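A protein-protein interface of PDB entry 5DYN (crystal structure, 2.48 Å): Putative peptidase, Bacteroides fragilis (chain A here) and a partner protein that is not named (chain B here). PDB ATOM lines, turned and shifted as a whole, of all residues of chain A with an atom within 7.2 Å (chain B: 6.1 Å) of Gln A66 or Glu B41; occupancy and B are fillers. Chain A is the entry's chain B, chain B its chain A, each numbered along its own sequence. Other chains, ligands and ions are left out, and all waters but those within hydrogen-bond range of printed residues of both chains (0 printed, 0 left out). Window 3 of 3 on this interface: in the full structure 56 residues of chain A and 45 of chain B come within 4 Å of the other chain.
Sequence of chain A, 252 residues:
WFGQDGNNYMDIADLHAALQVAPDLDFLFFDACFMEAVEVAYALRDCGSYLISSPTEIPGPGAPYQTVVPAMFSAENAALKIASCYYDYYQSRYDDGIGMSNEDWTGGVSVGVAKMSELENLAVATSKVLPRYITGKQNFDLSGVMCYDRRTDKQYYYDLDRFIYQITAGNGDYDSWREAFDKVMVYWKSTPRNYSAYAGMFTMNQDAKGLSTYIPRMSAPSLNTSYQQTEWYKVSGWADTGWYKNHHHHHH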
ATOM      1  N   ALA A  63     -29.224  20.580  19.881  1.00  0.00           N
ATOM      2  CA  ALA A  63     -29.038  20.843  18.461  1.00  0.00           C
ATOM      3  C   ALA A  63     -28.830  19.559  17.661  1.00  0.00           C
ATOM      4  O   ALA A  63     -28.229  18.603  18.155  1.00  0.00           O
ATOM      5  CB  ALA A  63     -27.859  21.787  18.255  1.00  0.00           C
ATOM      6  N   PRO A  64     -29.346  19.533  16.421  1.00  0.00           N
ATOM      7  CA  PRO A  64     -28.996  18.489  15.453  1.00  0.00           C
ATOM      8  C   PRO A  64     -27.605  18.756  14.902  1.00  0.00           C
ATOM      9  O   PRO A  64     -27.462  19.277  13.796  1.00  0.00           O
ATOM     10  CB  PRO A  64     -30.066  18.635  14.371  1.00  0.00           C
ATOM     11  CG  PRO A  64     -30.444  20.079  14.431  1.00  0.00           C
ATOM     12  CD  PRO A  64     -30.347  20.470  15.882  1.00  0.00           C
ATOM     13  N   TYR A  65     -26.585  18.402  15.677  1.00  0.00           N
ATOM     14  CA  TYR A  65     -25.210  18.757  15.342  1.00  0.00           C
ATOM     15  C   TYR A  65     -24.716  18.110  14.051  1.00  0.00           C
ATOM     16  O   TYR A  65     -23.630  18.431  13.574  1.00  0.00           O
ATOM     17  CB  TYR A  65     -24.277  18.397  16.503  1.00  0.00           C
ATOM     18  CG  TYR A  65     -24.419  19.325  17.690  1.00  0.00           C
ATOM     19  CD1 TYR A  65     -23.845  20.592  17.676  1.00  0.00           C
ATOM     20  CD2 TYR A  65     -25.129  18.941  18.820  1.00  0.00           C
ATOM     21  CE1 TYR A  65     -23.977  21.450  18.752  1.00  0.00           C
ATOM     22  CE2 TYR A  65     -25.264  19.793  19.903  1.00  0.00           C
ATOM     23  CZ  TYR A  65     -24.685  21.046  19.863  1.00  0.00           C
ATOM     24  OH  TYR A  65     -24.814  21.901  20.935  1.00  0.00           O
ATOM     25  N   GLN A  66     -25.508  17.209  13.478  1.00  0.00           N
ATOM     26  CA  GLN A  66     -25.169  16.649  12.177  1.00  0.00           C
ATOM     27  C   GLN A  66     -25.377  17.703  11.089  1.00  0.00           C
ATOM     28  O   GLN A  66     -24.730  17.661  10.044  1.00  0.00           O
ATOM     29  CB  GLN A  66     -25.993  15.392  11.880  1.00  0.00           C
ATOM     30  CG  GLN A  66     -27.495  15.603  11.841  1.00  0.00           C
ATOM     31  CD  GLN A  66     -28.164  15.314  13.170  1.00  0.00           C
ATOM     32  OE1 GLN A  66     -27.564  15.475  14.231  1.00  0.00           O
ATOM     33  NE2 GLN A  66     -29.416  14.880  13.115  1.00  0.00           N
ATOM     34  N   THR A  67     -26.271  18.655  11.346  1.00  0.00           N
ATOM     35  CA  THR A  67     -26.505  19.752  10.411  1.00  0.00           C
ATOM     36  C   THR A  67     -26.026  21.091  10.970  1.00  0.00           C
ATOM     37  O   THR A  67     -25.679  21.997  10.211  1.00  0.00           O
ATOM     38  CB  THR A  67     -27.990  19.877  10.046  1.00  0.00           C
ATOM     39  OG1 THR A  67     -28.744  20.225  11.212  1.00  0.00           O
ATOM     40  CG2 THR A  67     -28.512  18.567   9.472  1.00  0.00           C
ATOM     41  N   VAL A  68     -26.002  21.214  12.296  1.00  0.00           N
ATOM     42  CA  VAL A  68     -25.573  22.454  12.937  1.00  0.00           C
ATOM     43  C   VAL A  68     -24.066  22.654  12.783  1.00  0.00           C
ATOM     44  O   VAL A  68     -23.602  23.773  12.549  1.00  0.00           O
ATOM     45  CB  VAL A  68     -25.952  22.483  14.437  1.00  0.00           C
ATOM     46  CG1 VAL A  68     -25.367  23.712  15.116  1.00  0.00           C
ATOM     47  CG2 VAL A  68     -27.460  22.469  14.598  1.00  0.00           C
ATOM     48  N   VAL A  69     -23.302  21.571  12.898  1.00  0.00           N
ATOM     49  CA  VAL A  69     -21.853  21.666  12.738  1.00  0.00           C
ATOM     50  C   VAL A  69     -21.472  22.207  11.349  1.00  0.00           C
ATOM     51  O   VAL A  69     -20.657  23.122  11.263  1.00  0.00           O
ATOM     52  CB  VAL A  69     -21.150  20.306  12.999  1.00  0.00           C
ATOM     53  CG1 VAL A  69     -19.794  20.262  12.323  1.00  0.00           C
ATOM     54  CG2 VAL A  69     -21.014  20.054  14.491  1.00  0.00           C
ATOM     55  N   PRO A  70     -22.063  21.667  10.260  1.00  0.00           N
ATOM     56  CA  PRO A  70     -21.771  22.312   8.973  1.00  0.00           C
ATOM     57  C   PRO A  70     -22.221  23.773   8.920  1.00  0.00           C
ATOM     58  O   PRO A  70     -21.536  24.604   8.322  1.00  0.00           O
ATOM     59  CB  PRO A  70     -22.564  21.469   7.969  1.00  0.00           C
ATOM     60  CG  PRO A  70     -22.696  20.145   8.611  1.00  0.00           C
ATOM     61  CD  PRO A  70     -22.841  20.425  10.074  1.00  0.00           C
ATOM     62  N   ALA A  71     -23.356  24.078   9.543  1.00  0.00           N
ATOM     63  CA  ALA A  71     -23.852  25.449   9.596  1.00  0.00           C
ATOM     64  C   ALA A  71     -22.843  26.367  10.277  1.00  0.00           C
ATOM     65  O   ALA A  71     -22.682  27.522   9.887  1.00  0.00           O
ATOM     66  CB  ALA A  71     -25.189  25.506  10.317  1.00  0.00           C
ATOM     67  N   TYR A  89     -35.082  21.202  11.814  1.00  0.00           N
ATOM     68  CA  TYR A  89     -35.032  19.821  12.276  1.00  0.00           C
ATOM     69  C   TYR A  89     -36.235  19.471  13.139  1.00  0.00           C
ATOM     70  O   TYR A  89     -36.893  18.451  12.926  1.00  0.00           O
ATOM     71  CB  TYR A  89     -33.747  19.569  13.061  1.00  0.00           C
ATOM     72  CG  TYR A  89     -33.538  18.125  13.453  1.00  0.00           C
ATOM     73  CD1 TYR A  89     -32.868  17.250  12.608  1.00  0.00           C
ATOM     74  CD2 TYR A  89     -34.005  17.635  14.668  1.00  0.00           C
ATOM     75  CE1 TYR A  89     -32.669  15.927  12.959  1.00  0.00           C
ATOM     76  CE2 TYR A  89     -33.814  16.312  15.026  1.00  0.00           C
ATOM     77  CZ  TYR A  89     -33.144  15.464  14.168  1.00  0.00           C
ATOM     78  OH  TYR A  89     -32.944  14.147  14.515  1.00  0.00           O
ATOM     79  N   ARG A  93     -40.264  17.355  12.477  1.00  0.00           N
ATOM     80  CA  ARG A  93     -40.728  16.242  13.293  1.00  0.00           C
ATOM     81  C   ARG A  93     -41.794  16.686  14.293  1.00  0.00           C
ATOM     82  O   ARG A  93     -42.204  15.916  15.160  1.00  0.00           O
ATOM     83  CB  ARG A  93     -39.543  15.601  14.016  1.00  0.00           C
ATOM     84  CG  ARG A  93     -38.522  15.001  13.062  1.00  0.00           C
ATOM     85  CD  ARG A  93     -37.182  14.749  13.727  1.00  0.00           C
ATOM     86  NE  ARG A  93     -36.258  14.080  12.815  1.00  0.00           N
ATOM     87  CZ  ARG A  93     -35.589  14.695  11.845  1.00  0.00           C
ATOM     88  NH1 ARG A  93     -35.735  16.000  11.660  1.00  0.00           N
ATOM     89  NH2 ARG A  93     -34.772  14.006  11.059  1.00  0.00           N
ATOM     90  N   ILE B  36     -22.060  14.659  20.649  1.00  0.00           N
ATOM     91  CA  ILE B  36     -20.679  14.546  20.193  1.00  0.00           C
ATOM     92  C   ILE B  36     -20.593  13.653  18.956  1.00  0.00           C
ATOM     93  O   ILE B  36     -19.858  13.950  18.013  1.00  0.00           O
ATOM     94  CB  ILE B  36     -19.756  13.991  21.300  1.00  0.00           C
ATOM     95  CG1 ILE B  36     -19.714  14.957  22.486  1.00  0.00           C
ATOM     96  CG2 ILE B  36     -18.353  13.757  20.763  1.00  0.00           C
ATOM     97  CD1 ILE B  36     -18.669  14.617  23.535  1.00  0.00           C
ATOM     98  N   GLU B  37     -21.358  12.566  18.954  1.00  0.00           N
ATOM     99  CA  GLU B  37     -21.392  11.679  17.799  1.00  0.00           C
ATOM    100  C   GLU B  37     -22.033  12.387  16.609  1.00  0.00           C
ATOM    101  O   GLU B  37     -21.585  12.234  15.472  1.00  0.00           O
ATOM    102  CB  GLU B  37     -22.143  10.387  18.130  1.00  0.00           C
ATOM    103  CG  GLU B  37     -21.473   9.556  19.224  1.00  0.00           C
ATOM    104  CD  GLU B  37     -20.133   8.967  18.803  1.00  0.00           C
ATOM    105  OE1 GLU B  37     -19.853   8.906  17.586  1.00  0.00           O
ATOM    106  OE2 GLU B  37     -19.350   8.576  19.696  1.00  0.00           O
ATOM    107  N   GLU B  38     -23.070  13.174  16.877  1.00  0.00           N
ATOM    108  CA  GLU B  38     -23.702  13.984  15.842  1.00  0.00           C
ATOM    109  C   GLU B  38     -22.719  15.005  15.273  1.00  0.00           C
ATOM    110  O   GLU B  38     -22.788  15.362  14.097  1.00  0.00           O
ATOM    111  CB  GLU B  38     -24.935  14.696  16.393  1.00  0.00           C
ATOM    112  CG  GLU B  38     -26.100  13.780  16.711  1.00  0.00           C
ATOM    113  CD  GLU B  38     -27.247  14.518  17.373  1.00  0.00           C
ATOM    114  OE1 GLU B  38     -27.229  15.768  17.377  1.00  0.00           O
ATOM    115  OE2 GLU B  38     -28.160  13.852  17.900  1.00  0.00           O
ATOM    116  N   MET B  39     -21.805  15.473  16.115  1.00  0.00           N
ATOM    117  CA  MET B  39     -20.791  16.423  15.679  1.00  0.00           C
ATOM    118  C   MET B  39     -19.819  15.773  14.700  1.00  0.00           C
ATOM    119  O   MET B  39     -19.473  16.367  13.679  1.00  0.00           O
ATOM    120  CB  MET B  39     -20.039  16.994  16.882  1.00  0.00           C
ATOM    121  CG  MET B  39     -20.902  17.877  17.762  1.00  0.00           C
ATOM    122  SD  MET B  39     -20.128  18.404  19.302  1.00  0.00           S
ATOM    123  CE  MET B  39     -21.538  19.191  20.085  1.00  0.00           C
ATOM    124  N   LYS B  40     -19.382  14.557  15.015  1.00  0.00           N
ATOM    125  CA  LYS B  40     -18.511  13.800  14.119  1.00  0.00           C
ATOM    126  C   LYS B  40     -19.176  13.609  12.765  1.00  0.00           C
ATOM    127  O   LYS B  40     -18.569  13.843  11.721  1.00  0.00           O
ATOM    128  CB  LYS B  40     -18.165  12.437  14.718  1.00  0.00           C
ATOM    129  CG  LYS B  40     -17.336  12.492  15.982  1.00  0.00           C
ATOM    130  CD  LYS B  40     -17.107  11.095  16.523  1.00  0.00           C
ATOM    131  CE  LYS B  40     -16.527  11.140  17.918  1.00  0.00           C
ATOM    132  NZ  LYS B  40     -16.364   9.775  18.489  1.00  0.00           N
ATOM    133  N   GLU B  41     -20.433  13.181  12.801  1.00  0.00           N
ATOM    134  CA  GLU B  41     -21.228  12.986  11.598  1.00  0.00           C
ATOM    135  C   GLU B  41     -21.345  14.275  10.788  1.00  0.00           C
ATOM    136  O   GLU B  41     -21.209  14.265   9.565  1.00  0.00           O
ATOM    137  CB  GLU B  41     -22.613  12.464  11.972  1.00  0.00           C
ATOM    138  CG  GLU B  41     -23.625  12.475  10.846  1.00  0.00           C
ATOM    139  CD  GLU B  41     -24.887  11.719  11.209  1.00  0.00           C
ATOM    140  OE1 GLU B  41     -24.965  11.217  12.353  1.00  0.00           O
ATOM    141  OE2 GLU B  41     -25.800  11.632  10.358  1.00  0.00           O
ATOM    142  N   GLY B  42     -21.592  15.387  11.476  1.00  0.00           N
ATOM    143  CA  GLY B  42     -21.703  16.676  10.815  1.00  0.00           C
ATOM    144  C   GLY B  42     -20.356  17.162  10.315  1.00  0.00           C
ATOM    145  O   GLY B  42     -20.266  17.885   9.323  1.00  0.00           O
ATOM    146  N   MET B  43     -19.303  16.751  11.008  1.00  0.00           N
ATOM    147  CA  MET B  43     -17.945  17.140  10.653  1.00  0.00           C
ATOM    148  C   MET B  43     -17.516  16.512   9.327  1.00  0.00           C
ATOM    149  O   MET B  43     -16.564  16.967   8.690  1.00  0.00           O
ATOM    150  CB  MET B  43     -16.985  16.748  11.781  1.00  0.00           C
ATOM    151  CG  MET B  43     -15.559  17.233  11.619  1.00  0.00           C
ATOM    152  SD  MET B  43     -15.421  18.923  11.010  1.00  0.00           S
ATOM    153  CE  MET B  43     -16.304  19.825  12.258  1.00  0.00           C
ATOM    154  N   ARG B  44     -18.238  15.476   8.909  1.00  0.00           N
ATOM    155  CA  ARG B  44     -17.932  14.770   7.669  1.00  0.00           C
ATOM    156  C   ARG B  44     -18.085  15.671   6.449  1.00  0.00           C
ATOM    157  O   ARG B  44     -17.242  15.661   5.553  1.00  0.00           O
ATOM    158  CB  ARG B  44     -18.825  13.536   7.527  1.00  0.00           C
ATOM    159  CG  ARG B  44     -18.471  12.411   8.486  1.00  0.00           C
ATOM    160  CD  ARG B  44     -19.527  11.317   8.502  1.00  0.00           C
ATOM    161  NE  ARG B  44     -19.789  10.771   7.174  1.00  0.00           N
ATOM    162  CZ  ARG B  44     -20.895  11.004   6.474  1.00  0.00           C
ATOM    163  NH1 ARG B  44     -21.851  11.775   6.973  1.00  0.00           N
ATOM    164  NH2 ARG B  44     -21.047  10.462   5.273  1.00  0.00           N
ATOM    165  N   GLN B  45     -19.161  16.449   6.413  1.00  0.00           N
ATOM    166  CA  GLN B  45     -19.374  17.373   5.306  1.00  0.00           C
ATOM    167  C   GLN B  45     -18.775  18.741   5.622  1.00  0.00           C
ATOM    168  O   GLN B  45     -19.310  19.771   5.215  1.00  0.00           O
ATOM    169  CB  GLN B  45     -20.866  17.496   4.985  1.00  0.00           C
ATOM    170  CG  GLN B  45     -21.507  16.182   4.551  1.00  0.00           C
ATOM    171  CD  GLN B  45     -22.153  16.261   3.175  1.00  0.00           C
ATOM    172  OE1 GLN B  45     -22.872  17.213   2.866  1.00  0.00           O
ATOM    173  NE2 GLN B  45     -21.898  15.257   2.341  1.00  0.00           N
ATOM    174  N   VAL B  76     -13.686  10.739  10.299  1.00  0.00           N
ATOM    175  CA  VAL B  76     -13.641  11.664  11.426  1.00  0.00           C
ATOM    176  C   VAL B  76     -13.063  10.979  12.661  1.00  0.00           C
ATOM    177  O   VAL B  76     -13.521   9.907  13.056  1.00  0.00           O
ATOM    178  CB  VAL B  76     -15.039  12.227  11.755  1.00  0.00           C
ATOM    179  CG1 VAL B  76     -15.002  13.033  13.045  1.00  0.00           C
ATOM    180  CG2 VAL B  76     -15.546  13.081  10.602  1.00  0.00           C
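The backbone carbonyl oxygen of Pro A64 sits at hydrogen-bond distance from the side-chain hydroxyl of Thr A67 (3.0 Å).
OE1 of Glu B38 is in hydrogen-bond range of N of Tyr A65 (3.2 Å).
The side-chain carboxylate (OE1) of Glu B38 lies close to the side-chain amide oxygen (OE1) of Gln A66 (3.2 Å).
The backbone carbonyl oxygen (O) of Ala A63 lies close to the side-chain carboxylate (OE1) of Glu B38.
Among the printed residues, merely in contact across the chains: Gln A66 with Gly B42 (3.3 Å), Pro A70 with Gly B42 (3.4 Å), Val A69 with Met B43 (3.5 Å), Tyr A65 with Met B39 (3.6 Å), Val A69 with Gly B42 (3.7 Å), Pro A64 with Glu B38 (3.8 Å), Tyr A65 with Gly B42 (3.8 Å), Val A69 with Met B39 (3.8 Å) and Gln A66 with Glu B41 (3.9 Å).
Of the printed residues of chain B, Tyr A65 touches Glu B38, Met B39 and Gly B42.
Gln A66 touches just these residues of chain B: Glu B38, Glu B41 and Gly B42.
Printed residues of chain B within 4 Å of Pro A70: Gly B42.
Printed residues of chain A within 4 Å of Glu B38: Ala A63, Pro A64, Tyr A65 and Gln A66.
Of the printed residues of chain A, Met B39 touches Tyr A65 (3.6 Å) and Val A69 (3.8 Å).
Of the printed residues of chain A, Glu B41 touches Gln A66.
Of the printed residues of chain A, Met B43 touches Val A69.
The nearest residue of chain A that does not touch Glu B41 is Tyr A65 (5.5 Å).
Of the 11 printed residues of chain B, 5 touch a printed residue of chain A.
Printed residues of chain B that touch a printed residue of chain A: Glu B38, Met B39, Glu B41, Gly B42 and Met B43.
Hydrophobic or aromatic side chains of chain B that line the printed part of chain A: Met B39 and Met B43.
Of the 11 printed residues of chain A, 6 touch a printed residue of chain B.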
